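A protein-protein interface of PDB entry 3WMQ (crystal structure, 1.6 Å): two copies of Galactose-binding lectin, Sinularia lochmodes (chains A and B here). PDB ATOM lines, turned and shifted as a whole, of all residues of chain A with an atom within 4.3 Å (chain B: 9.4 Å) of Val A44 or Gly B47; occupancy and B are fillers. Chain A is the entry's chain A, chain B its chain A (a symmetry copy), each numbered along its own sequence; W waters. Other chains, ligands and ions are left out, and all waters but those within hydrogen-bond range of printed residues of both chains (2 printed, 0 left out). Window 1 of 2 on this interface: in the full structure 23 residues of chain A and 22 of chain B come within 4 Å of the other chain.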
ATOM      1  N   ILE A  43     -31.570  -4.146  -5.240  1.00  0.00           N
ATOM      2  CA  ILE A  43     -31.101  -2.862  -5.745  1.00  0.00           C
ATOM      3  C   ILE A  43     -32.189  -2.311  -6.642  1.00  0.00           C
ATOM      4  O   ILE A  43     -32.953  -3.063  -7.251  1.00  0.00           O
ATOM      5  CB  ILE A  43     -29.742  -2.925  -6.509  1.00  0.00           C
ATOM      6  CG1 ILE A  43     -29.783  -3.947  -7.646  1.00  0.00           C
ATOM      7  CG2 ILE A  43     -28.612  -3.173  -5.527  1.00  0.00           C
ATOM      8  CD1 ILE A  43     -28.521  -3.932  -8.485  1.00  0.00           C
ATOM      9  N   VAL A  44     -32.266  -0.987  -6.695  1.00  0.00           N
ATOM     10  CA  VAL A  44     -33.301  -0.307  -7.463  1.00  0.00           C
ATOM     11  C   VAL A  44     -32.714   0.797  -8.352  1.00  0.00           C
ATOM     12  O   VAL A  44     -31.770   1.480  -7.962  1.00  0.00           O
ATOM     13  CB  VAL A  44     -34.319   0.343  -6.493  1.00  0.00           C
ATOM     14  CG1 VAL A  44     -35.489   0.937  -7.258  1.00  0.00           C
ATOM     15  CG2 VAL A  44     -34.807  -0.690  -5.475  1.00  0.00           C
ATOM     16  N   SER A  45     -33.261   0.960  -9.552  1.00  0.00           N
ATOM     17  CA  SER A  45     -32.804   2.024 -10.445  1.00  0.00           C
ATOM     18  C   SER A  45     -33.993   2.537 -11.240  1.00  0.00           C
ATOM     19  O   SER A  45     -35.143   2.268 -10.898  1.00  0.00           O
ATOM     20  CB  SER A  45     -31.701   1.546 -11.400  1.00  0.00           C
ATOM     21  OG  SER A  45     -31.141   2.652 -12.105  1.00  0.00           O
ATOM     22  N   PHE A  46     -33.707   3.280 -12.301  1.00  0.00           N
ATOM     23  CA  PHE A  46     -34.751   3.855 -13.136  1.00  0.00           C
ATOM     24  C   PHE A  46     -34.676   3.327 -14.561  1.00  0.00           C
ATOM     25  O   PHE A  46     -33.612   3.344 -15.176  1.00  0.00           O
ATOM     26  CB  PHE A  46     -34.610   5.384 -13.150  1.00  0.00           C
ATOM     27  CG  PHE A  46     -34.922   6.030 -11.832  1.00  0.00           C
ATOM     28  CD1 PHE A  46     -36.205   6.494 -11.557  1.00  0.00           C
ATOM     29  CD2 PHE A  46     -33.941   6.147 -10.847  1.00  0.00           C
ATOM     30  CE1 PHE A  46     -36.510   7.068 -10.320  1.00  0.00           C
ATOM     31  CE2 PHE A  46     -34.236   6.719  -9.604  1.00  0.00           C
ATOM     32  CZ  PHE A  46     -35.523   7.178  -9.343  1.00  0.00           C
ATOM     33  N   ASN A  60     -34.327   9.723  -6.264  1.00  0.00           N
ATOM     34  CA  ASN A  60     -33.824   8.746  -5.311  1.00  0.00           C
ATOM     35  C   ASN A  60     -34.710   7.503  -5.320  1.00  0.00           C
ATOM     36  O   ASN A  60     -35.915   7.592  -5.541  1.00  0.00           O
ATOM     37  CB  ASN A  60     -33.818   9.392  -3.924  1.00  0.00           C
ATOM     38  CG  ASN A  60     -33.254   8.493  -2.850  1.00  0.00           C
ATOM     39  OD1 ASN A  60     -32.198   7.869  -3.015  1.00  0.00           O
ATOM     40  ND2 ASN A  60     -33.957   8.472  -1.721  1.00  0.00           N
ATOM     41  N   SER A  61     -34.101   6.344  -5.098  1.00  0.00           N
ATOM     42  CA  SER A  61     -34.841   5.088  -5.052  1.00  0.00           C
ATOM     43  C   SER A  61     -34.102   4.171  -4.096  1.00  0.00           C
ATOM     44  O   SER A  61     -32.881   4.273  -3.944  1.00  0.00           O
ATOM     45  CB  SER A  61     -34.928   4.442  -6.441  1.00  0.00           C
ATOM     46  OG  SER A  61     -33.659   4.004  -6.895  1.00  0.00           O
ATOM     47  N   SER A  62     -34.847   3.281  -3.450  1.00  0.00           N
ATOM     48  CA  SER A  62     -34.249   2.351  -2.503  1.00  0.00           C
ATOM     49  C   SER A  62     -35.192   1.198  -2.213  1.00  0.00           C
ATOM     50  O   SER A  62     -36.377   1.262  -2.517  1.00  0.00           O
ATOM     51  CB  SER A  62     -33.920   3.073  -1.190  1.00  0.00           C
ATOM     52  OG  SER A  62     -35.091   3.539  -0.548  1.00  0.00           O
ATOM     53  N   ALA A  63     -34.643   0.138  -1.634  1.00  0.00           N
ATOM     54  CA  ALA A  63     -35.431  -1.020  -1.243  1.00  0.00           C
ATOM     55  C   ALA A  63     -35.362  -0.960   0.273  1.00  0.00           C
ATOM     56  O   ALA A  63     -34.287  -1.107   0.855  1.00  0.00           O
ATOM     57  CB  ALA A  63     -34.793  -2.312  -1.770  1.00  0.00           C
ATOM     58  N   LEU A  73     -40.724  -0.826  -1.974  1.00  0.00           N
ATOM     59  CA  LEU A  73     -40.079  -0.170  -3.105  1.00  0.00           C
ATOM     60  C   LEU A  73     -40.281   1.328  -2.917  1.00  0.00           C
ATOM     61  O   LEU A  73     -41.403   1.827  -3.002  1.00  0.00           O
ATOM     62  CB  LEU A  73     -40.718  -0.640  -4.408  1.00  0.00           C
ATOM     63  CG  LEU A  73     -40.227  -0.003  -5.706  1.00  0.00           C
ATOM     64  CD1 LEU A  73     -38.751  -0.291  -5.900  1.00  0.00           C
ATOM     65  CD2 LEU A  73     -41.036  -0.552  -6.868  1.00  0.00           C
ATOM     66  N   ILE A  89     -37.039   0.102 -11.624  1.00  0.00           N
ATOM     67  CA  ILE A  89     -36.718  -1.282 -11.940  1.00  0.00           C
ATOM     68  C   ILE A  89     -36.023  -1.765 -10.691  1.00  0.00           C
ATOM     69  O   ILE A  89     -35.350  -0.991 -10.005  1.00  0.00           O
ATOM     70  CB  ILE A  89     -35.763  -1.467 -13.170  1.00  0.00           C
ATOM     71  CG1 ILE A  89     -34.395  -0.841 -12.900  1.00  0.00           C
ATOM     72  CG2 ILE A  89     -36.411  -0.933 -14.424  1.00  0.00           C
ATOM     73  CD1 ILE A  89     -33.322  -1.329 -13.858  1.00  0.00           C
ATOM     74  N   TRP A  90     -36.209  -3.038 -10.367  1.00  0.00           N
ATOM     75  CA  TRP A  90     -35.581  -3.574  -9.174  1.00  0.00           C
ATOM     76  C   TRP A  90     -35.255  -5.040  -9.344  1.00  0.00           C
ATOM     77  O   TRP A  90     -35.887  -5.739 -10.131  1.00  0.00           O
ATOM     78  CB  TRP A  90     -36.491  -3.401  -7.948  1.00  0.00           C
ATOM     79  CG  TRP A  90     -37.822  -4.093  -8.059  1.00  0.00           C
ATOM     80  CD1 TRP A  90     -38.996  -3.552  -8.496  1.00  0.00           C
ATOM     81  CD2 TRP A  90     -38.105  -5.466  -7.747  1.00  0.00           C
ATOM     82  NE1 TRP A  90     -39.995  -4.499  -8.475  1.00  0.00           N
ATOM     83  CE2 TRP A  90     -39.475  -5.681  -8.021  1.00  0.00           C
ATOM     84  CE3 TRP A  90     -37.335  -6.532  -7.263  1.00  0.00           C
ATOM     85  CZ2 TRP A  90     -40.093  -6.927  -7.828  1.00  0.00           C
ATOM     86  CZ3 TRP A  90     -37.951  -7.770  -7.070  1.00  0.00           C
ATOM     87  CH2 TRP A  90     -39.316  -7.953  -7.354  1.00  0.00           C
ATOM     88  N   MET B  10     -24.418  -8.122  -5.169  1.00  0.00           N
ATOM     89  CA  MET B  10     -24.823  -6.784  -5.566  1.00  0.00           C
ATOM     90  C   MET B  10     -24.530  -5.798  -4.458  1.00  0.00           C
ATOM     91  O   MET B  10     -24.268  -6.183  -3.318  1.00  0.00           O
ATOM     92  CB  MET B  10     -26.314  -6.752  -5.929  1.00  0.00           C
ATOM     93  CG  MET B  10     -27.278  -6.919  -4.763  1.00  0.00           C
ATOM     94  SD  MET B  10     -28.995  -6.919  -5.328  1.00  0.00           S
ATOM     95  CE  MET B  10     -29.106  -8.570  -5.986  1.00  0.00           C
ATOM     96  N   GLY B  11     -24.556  -4.517  -4.792  1.00  0.00           N
ATOM     97  CA  GLY B  11     -24.287  -3.526  -3.777  1.00  0.00           C
ATOM     98  C   GLY B  11     -24.563  -2.120  -4.258  1.00  0.00           C
ATOM     99  O   GLY B  11     -24.941  -1.906  -5.406  1.00  0.00           O
ATOM    100  N   THR B  12     -24.367  -1.163  -3.359  1.00  0.00           N
ATOM    101  CA  THR B  12     -24.579   0.244  -3.667  1.00  0.00           C
ATOM    102  C   THR B  12     -23.433   1.047  -3.072  1.00  0.00           C
ATOM    103  O   THR B  12     -22.776   0.605  -2.131  1.00  0.00           O
ATOM    104  CB  THR B  12     -25.911   0.772  -3.069  1.00  0.00           C
ATOM    105  OG1 THR B  12     -25.825   0.787  -1.638  1.00  0.00           O
ATOM    106  CG2 THR B  12     -27.085  -0.098  -3.491  1.00  0.00           C
ATOM    107  N   SER B  13     -23.187   2.223  -3.634  1.00  0.00           N
ATOM    108  CA  SER B  13     -22.139   3.093  -3.126  1.00  0.00           C
ATOM    109  C   SER B  13     -22.677   4.509  -3.205  1.00  0.00           C
ATOM    110  O   SER B  13     -22.857   5.061  -4.294  1.00  0.00           O
ATOM    111  CB  SER B  13     -20.855   2.974  -3.947  1.00  0.00           C
ATOM    112  OG  SER B  13     -19.849   3.810  -3.395  1.00  0.00           O
ATOM    113  N   THR B  14     -22.944   5.083  -2.038  1.00  0.00           N
ATOM    114  CA  THR B  14     -23.504   6.426  -1.953  1.00  0.00           C
ATOM    115  C   THR B  14     -22.465   7.532  -1.794  1.00  0.00           C
ATOM    116  O   THR B  14     -21.587   7.474  -0.922  1.00  0.00           O
ATOM    117  CB  THR B  14     -24.500   6.527  -0.780  1.00  0.00           C
ATOM    118  OG1 THR B  14     -25.573   5.602  -0.994  1.00  0.00           O
ATOM    119  CG2 THR B  14     -25.062   7.944  -0.672  1.00  0.00           C
ATOM    120  N   VAL B  44     -23.462  -1.716 -13.943  1.00  0.00           N
ATOM    121  CA  VAL B  44     -23.585  -0.629 -12.980  1.00  0.00           C
ATOM    122  C   VAL B  44     -24.587   0.434 -13.450  1.00  0.00           C
ATOM    123  O   VAL B  44     -24.675   0.730 -14.639  1.00  0.00           O
ATOM    124  CB  VAL B  44     -22.206   0.053 -12.796  1.00  0.00           C
ATOM    125  CG1 VAL B  44     -22.264   1.096 -11.693  1.00  0.00           C
ATOM    126  CG2 VAL B  44     -21.137  -0.998 -12.490  1.00  0.00           C
ATOM    127  N   SER B  45     -25.352   0.994 -12.520  1.00  0.00           N
ATOM    128  CA  SER B  45     -26.296   2.056 -12.865  1.00  0.00           C
ATOM    129  C   SER B  45     -26.375   3.035 -11.706  1.00  0.00           C
ATOM    130  O   SER B  45     -25.527   3.026 -10.815  1.00  0.00           O
ATOM    131  CB  SER B  45     -27.694   1.508 -13.186  1.00  0.00           C
ATOM    132  OG  SER B  45     -28.522   2.541 -13.716  1.00  0.00           O
ATOM    133  N   PHE B  46     -27.397   3.879 -11.725  1.00  0.00           N
ATOM    134  CA  PHE B  46     -27.579   4.885 -10.689  1.00  0.00           C
ATOM    135  C   PHE B  46     -28.883   4.674  -9.934  1.00  0.00           C
ATOM    136  O   PHE B  46     -29.940   4.528 -10.544  1.00  0.00           O
ATOM    137  CB  PHE B  46     -27.579   6.281 -11.327  1.00  0.00           C
ATOM    138  CG  PHE B  46     -26.245   6.691 -11.879  1.00  0.00           C
ATOM    139  CD1 PHE B  46     -25.351   7.420 -11.101  1.00  0.00           C
ATOM    140  CD2 PHE B  46     -25.864   6.319 -13.169  1.00  0.00           C
ATOM    141  CE1 PHE B  46     -24.094   7.778 -11.598  1.00  0.00           C
ATOM    142  CE2 PHE B  46     -24.608   6.671 -13.675  1.00  0.00           C
ATOM    143  CZ  PHE B  46     -23.725   7.400 -12.887  1.00  0.00           C
ATOM    144  N   GLY B  47     -28.806   4.683  -8.606  1.00  0.00           N
ATOM    145  CA  GLY B  47     -29.990   4.514  -7.783  1.00  0.00           C
ATOM    146  C   GLY B  47     -30.496   5.857  -7.286  1.00  0.00           C
ATOM    147  O   GLY B  47     -31.661   5.997  -6.920  1.00  0.00           O
ATOM    148  N   MET B  48     -29.606   6.844  -7.277  1.00  0.00           N
ATOM    149  CA  MET B  48     -29.932   8.201  -6.844  1.00  0.00           C
ATOM    150  C   MET B  48     -29.017   9.126  -7.633  1.00  0.00           C
ATOM    151  O   MET B  48     -27.860   8.792  -7.891  1.00  0.00           O
ATOM    152  CB  MET B  48     -29.696   8.358  -5.331  1.00  0.00           C
ATOM    153  CG  MET B  48     -29.924   9.763  -4.764  1.00  0.00           C
ATOM    154  SD  MET B  48     -28.445  10.798  -4.815  1.00  0.00           S
ATOM    155  CE  MET B  48     -27.537  10.157  -3.395  1.00  0.00           C
ATOM    156  N   LEU B  49     -29.542  10.280  -8.032  1.00  0.00           N
ATOM    157  CA  LEU B  49     -28.761  11.236  -8.808  1.00  0.00           C
ATOM    158  C   LEU B  49     -29.261  12.652  -8.542  1.00  0.00           C
ATOM    159  O   LEU B  49     -30.463  12.886  -8.463  1.00  0.00           O
ATOM    160  CB  LEU B  49     -28.876  10.908 -10.300  1.00  0.00           C
ATOM    161  CG  LEU B  49     -27.957  11.666 -11.252  1.00  0.00           C
ATOM    162  CD1 LEU B  49     -26.499  11.433 -10.852  1.00  0.00           C
ATOM    163  CD2 LEU B  49     -28.193  11.187 -12.681  1.00  0.00           C
ATOM    164  N   ASP B  50     -28.319  13.581  -8.412  1.00  0.00           N
ATOM    165  CA  ASP B  50     -28.594  14.992  -8.147  1.00  0.00           C
ATOM    166  C   ASP B  50     -27.660  15.751  -9.096  1.00  0.00           C
ATOM    167  O   ASP B  50     -26.455  15.859  -8.846  1.00  0.00           O
ATOM    168  CB  ASP B  50     -28.286  15.269  -6.667  1.00  0.00           C
ATOM    169  CG  ASP B  50     -28.583  16.695  -6.242  1.00  0.00           C
ATOM    170  OD1 ASP B  50     -28.582  16.941  -5.013  1.00  0.00           O
ATOM    171  OD2 ASP B  50     -28.794  17.564  -7.109  1.00  0.00           O
ATOM    172  N   VAL B  59     -23.372  11.647 -17.093  1.00  0.00           N
ATOM    173  CA  VAL B  59     -22.910  10.738 -16.051  1.00  0.00           C
ATOM    174  C   VAL B  59     -22.530   9.411 -16.688  1.00  0.00           C
ATOM    175  O   VAL B  59     -23.136   8.969 -17.670  1.00  0.00           O
ATOM    176  CB  VAL B  59     -23.960  10.510 -14.924  1.00  0.00           C
ATOM    177  CG1 VAL B  59     -24.255  11.836 -14.228  1.00  0.00           C
ATOM    178  CG2 VAL B  59     -25.230   9.877 -15.469  1.00  0.00           C
ATOM    179  N   SER B  61     -20.778   5.319 -15.666  1.00  0.00           N
ATOM    180  CA  SER B  61     -20.442   4.336 -14.643  1.00  0.00           C
ATOM    181  C   SER B  61     -20.023   3.068 -15.364  1.00  0.00           C
ATOM    182  O   SER B  61     -20.486   2.794 -16.474  1.00  0.00           O
ATOM    183  CB  SER B  61     -21.642   4.051 -13.729  1.00  0.00           C
ATOM    184  OG  SER B  61     -22.683   3.388 -14.424  1.00  0.00           O
ATOM    185  N   ASN B  85     -24.823  14.868  -5.825  1.00  0.00           N
ATOM    186  CA  ASN B  85     -25.010  13.638  -5.051  1.00  0.00           C
ATOM    187  C   ASN B  85     -25.296  12.515  -6.040  1.00  0.00           C
ATOM    188  O   ASN B  85     -25.869  12.756  -7.097  1.00  0.00           O
ATOM    189  CB  ASN B  85     -26.257  13.708  -4.140  1.00  0.00           C
ATOM    190  CG  ASN B  85     -26.129  14.688  -2.988  1.00  0.00           C
ATOM    191  OD1 ASN B  85     -25.331  14.494  -2.067  1.00  0.00           O
ATOM    192  ND2 ASN B  85     -26.953  15.730  -3.011  1.00  0.00           N
ATOM    193  N   TYR B  86     -24.921  11.288  -5.691  1.00  0.00           N
ATOM    194  CA  TYR B  86     -25.255  10.132  -6.527  1.00  0.00           C
ATOM    195  C   TYR B  86     -25.035   8.852  -5.756  1.00  0.00           C
ATOM    196  O   TYR B  86     -24.283   8.815  -4.784  1.00  0.00           O
ATOM    197  CB  TYR B  86     -24.469  10.097  -7.858  1.00  0.00           C
ATOM    198  CG  TYR B  86     -22.991   9.798  -7.764  1.00  0.00           C
ATOM    199  CD1 TYR B  86     -22.500   8.484  -7.766  1.00  0.00           C
ATOM    200  CD2 TYR B  86     -22.081  10.839  -7.687  1.00  0.00           C
ATOM    201  CE1 TYR B  86     -21.125   8.236  -7.696  1.00  0.00           C
ATOM    202  CE2 TYR B  86     -20.723  10.611  -7.615  1.00  0.00           C
ATOM    203  CZ  TYR B  86     -20.245   9.309  -7.618  1.00  0.00           C
ATOM    204  OH  TYR B  86     -18.890   9.098  -7.542  1.00  0.00           O
ATOM    205  N   LYS B  87     -25.747   7.816  -6.170  1.00  0.00           N
ATOM    206  CA  LYS B  87     -25.603   6.507  -5.560  1.00  0.00           C
ATOM    207  C   LYS B  87     -25.501   5.524  -6.694  1.00  0.00           C
ATOM    208  O   LYS B  87     -26.382   5.458  -7.547  1.00  0.00           O
ATOM    209  CB  LYS B  87     -26.803   6.131  -4.676  1.00  0.00           C
ATOM    210  CG  LYS B  87     -26.647   4.718  -4.064  1.00  0.00           C
ATOM    211  CD  LYS B  87     -27.776   4.359  -3.100  1.00  0.00           C
ATOM    212  CE  LYS B  87     -29.106   4.196  -3.827  1.00  0.00           C
ATOM    213  NZ  LYS B  87     -30.225   3.929  -2.874  1.00  0.00           N
ATOM    214  N   LEU B  88     -24.411   4.768  -6.712  1.00  0.00           N
ATOM    215  CA  LEU B  88     -24.223   3.770  -7.747  1.00  0.00           C
ATOM    216  C   LEU B  88     -24.811   2.467  -7.257  1.00  0.00           C
ATOM    217  O   LEU B  88     -24.802   2.198  -6.060  1.00  0.00           O
ATOM    218  CB  LEU B  88     -22.735   3.537  -8.016  1.00  0.00           C
ATOM    219  CG  LEU B  88     -21.896   4.689  -8.558  1.00  0.00           C
ATOM    220  CD1 LEU B  88     -20.429   4.280  -8.657  1.00  0.00           C
ATOM    221  CD2 LEU B  88     -22.444   5.078  -9.915  1.00  0.00           C
ATOM    222  N   ILE B  89     -25.342   1.674  -8.179  1.00  0.00           N
ATOM    223  CA  ILE B  89     -25.850   0.356  -7.826  1.00  0.00           C
ATOM    224  C   ILE B  89     -25.131  -0.555  -8.791  1.00  0.00           C
ATOM    225  O   ILE B  89     -24.825  -0.162  -9.919  1.00  0.00           O
ATOM    226  CB  ILE B  89     -27.398   0.183  -8.003  1.00  0.00           C
ATOM    227  CG1 ILE B  89     -27.802   0.335  -9.469  1.00  0.00           C
ATOM    228  CG2 ILE B  89     -28.141   1.130  -7.093  1.00  0.00           C
ATOM    229  CD1 ILE B  89     -29.188  -0.213  -9.760  1.00  0.00           C
ATOM    230  N   TRP B  90     -24.827  -1.766  -8.342  1.00  0.00           N
ATOM    231  CA  TRP B  90     -24.127  -2.697  -9.208  1.00  0.00           C
ATOM    232  C   TRP B  90     -24.514  -4.124  -8.896  1.00  0.00           C
ATOM    233  O   TRP B  90     -24.925  -4.436  -7.782  1.00  0.00           O
ATOM    234  CB  TRP B  90     -22.605  -2.546  -9.063  1.00  0.00           C
ATOM    235  CG  TRP B  90     -22.085  -2.804  -7.675  1.00  0.00           C
ATOM    236  CD1 TRP B  90     -21.858  -1.880  -6.697  1.00  0.00           C
ATOM    237  CD2 TRP B  90     -21.748  -4.079  -7.107  1.00  0.00           C
ATOM    238  NE1 TRP B  90     -21.401  -2.496  -5.554  1.00  0.00           N
ATOM    239  CE2 TRP B  90     -21.325  -3.844  -5.778  1.00  0.00           C
ATOM    240  CE3 TRP B  90     -21.763  -5.393  -7.592  1.00  0.00           C
ATOM    241  CZ2 TRP B  90     -20.920  -4.883  -4.925  1.00  0.00           C
ATOM    242  CZ3 TRP B  90     -21.360  -6.425  -6.742  1.00  0.00           C
ATOM    243  CH2 TRP B  90     -20.945  -6.160  -5.424  1.00  0.00           C
ATOM    244  N   ILE B  91     -24.400  -4.983  -9.899  1.00  0.00           N
ATOM    245  CA  ILE B  91     -24.703  -6.390  -9.711  1.00  0.00           C
ATOM    246  C   ILE B  91     -23.755  -7.208 -10.571  1.00  0.00           C
ATOM    247  O   ILE B  91     -23.530  -6.910 -11.748  1.00  0.00           O
ATOM    248  CB  ILE B  91     -26.181  -6.727 -10.047  1.00  0.00           C
ATOM    249  CG1 ILE B  91     -26.414  -8.231  -9.863  1.00  0.00           C
ATOM    250  CG2 ILE B  91     -26.527  -6.295 -11.462  1.00  0.00           C
ATOM    251  CD1 ILE B  91     -27.864  -8.647  -9.930  1.00  0.00           C
HETATM  252  O   HOH W   1     -31.325   2.580  -5.539  1.00  0.00           O
HETATM  253  O   HOH W   2     -30.421   6.381  -1.759  1.00  0.00           O
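The side-chain hydroxyl (OG) of Ser A61 lies within hydrogen-bond range of the backbone carbonyl oxygen (O) of Gly B47, 2.8 Å away.
The backbone carbonyl oxygen (O) of Phe B46 is in hydrogen-bond range of the side-chain hydroxyl (OG) of Ser A45 (2.7 Å).
O of Ser A61 sits at hydrogen-bond distance from NZ of Lys B87 (2.9 Å).
The side-chain sulfur of Met B10 lies close to the backbone NH of Ile A43, at 3.8 Å.
The side-chain hydroxyl (OG) of Ser B45 lies within hydrogen-bond range of the side-chain hydroxyl (OG) of Ser A45.
The side-chain sulfur of Met B48 sits close to the backbone NH of Tyr B86 (3.7 Å).
The backbone carbonyl oxygen of Lys B87 lies within hydrogen-bond range of the backbone NH of Gly B47, at 2.8 Å.
O of Gly B11 is in hydrogen-bond range of N of Trp B90 (2.9 Å).
The backbone carbonyl oxygen (O) of Ile A89 is in hydrogen-bond range of the backbone NH (N) of Ser A45 (2.9 Å).
The backbone carbonyl oxygen (O) of Val A44 lies within hydrogen-bond range of the side-chain hydroxyl (OG) of Ser A61, 3.3 Å away.
O of Met B48 lies within hydrogen-bond range of N of Lys B87, at 2.9 Å.
CG2 of Ile A43 touches O of Gly B11, 3.9 Å away.
Ile A43 touches Thr B12 (CG2 to CG2, 3.99 Å).
CD1 of Ile B89 touches CD1 of Ile A43, 3.99 Å away.
Ile A43 touches Trp B90.
Ile A43 touches Ile B91 (CD1 to CB, 3.97 Å).
O of Val A44 touches CD1 of Ile B89, at 3.6 Å.
CD1 of Ile B89 touches CB of Ser A45, at 3.5 Å.
Phe A46 touches Gly B47 (CE2 to O, 3.8 Å).
Gly B47 touches Asn A60.
OD1 of Asn A60 touches CG of Met B48 (3.4 Å).
Printed residues of chain B within 4 Å of Val A44: Gly B47 and Ile B89.
Of chain B, only Ser B45, Phe B46 and Ile B89 come within 4 Å of Ser A45.
Of the printed residues of chain B, Asn A60 touches Gly B47 (3.8 Å) and Met B48 (3.4 Å).
Of chain B, only Gly B47 (2.8 Å) and Lys B87 (2.9 Å) come within 4 Å of Ser A61.
Printed residues of chain A within 4 Å of Thr B12: Ile A43.
Gly B47 touches just these residues of chain A: Val A44 (3.5 Å), Phe A46 (3.8 Å), Asn A60 (3.8 Å) and Ser A61 (2.8 Å).
Of the printed residues of chain A, Lys B87 touches Ser A61.
Of the 11 printed residues of chain A, 6 touch a printed residue of chain B.
Of the 21 printed residues of chain B, 11 touch a printed residue of chain A.
Printed residues of chain B that touch a printed residue of chain A: Met B10, Gly B11, Thr B12, Ser B45, Phe B46, Gly B47, Met B48, Lys B87, Ile B89, Trp B90 and Ile B91.
Hydrophobic or aromatic side chains of chain B within 4 Å of the printed part of chain A: Met B10, Met B48, Ile B89 and Ile B91.
Among the printed residues, no Asp or Glu carboxylate lies within 4 Å of a Lys or Arg side-chain nitrogen of the other chain.
Val A44 touches Ile B89, but with the chains exchanged Ile A89 does not touch Val B44 (8.9 Å).
Ser B45 touches its own counterpart, Ser A45.
Ser A45 touches Phe B46, but with the chains exchanged Phe A46 does not touch Ser B45 (5.4 Å).
Ser A45 touches Ile B89, but with the chains exchanged Ile A89 does not touch Ser B45 (6.2 Å).
Positions printed for both chains: 44, 45, 46, 61, 89 and 90.
Of the 16 pairs that touch across the chains among the printed residues, 1 has its exchanged pair printed and touching as well.
Water W2 lies within hydrogen-bond range of OD1 of Asn A60 and NZ of Lys B87.
Water W1 lies within hydrogen-bond range of O of Val A44 (2.7 Å), O of Ser A61 (2.8 Å) and NZ of Lys B87 (3.2 Å).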
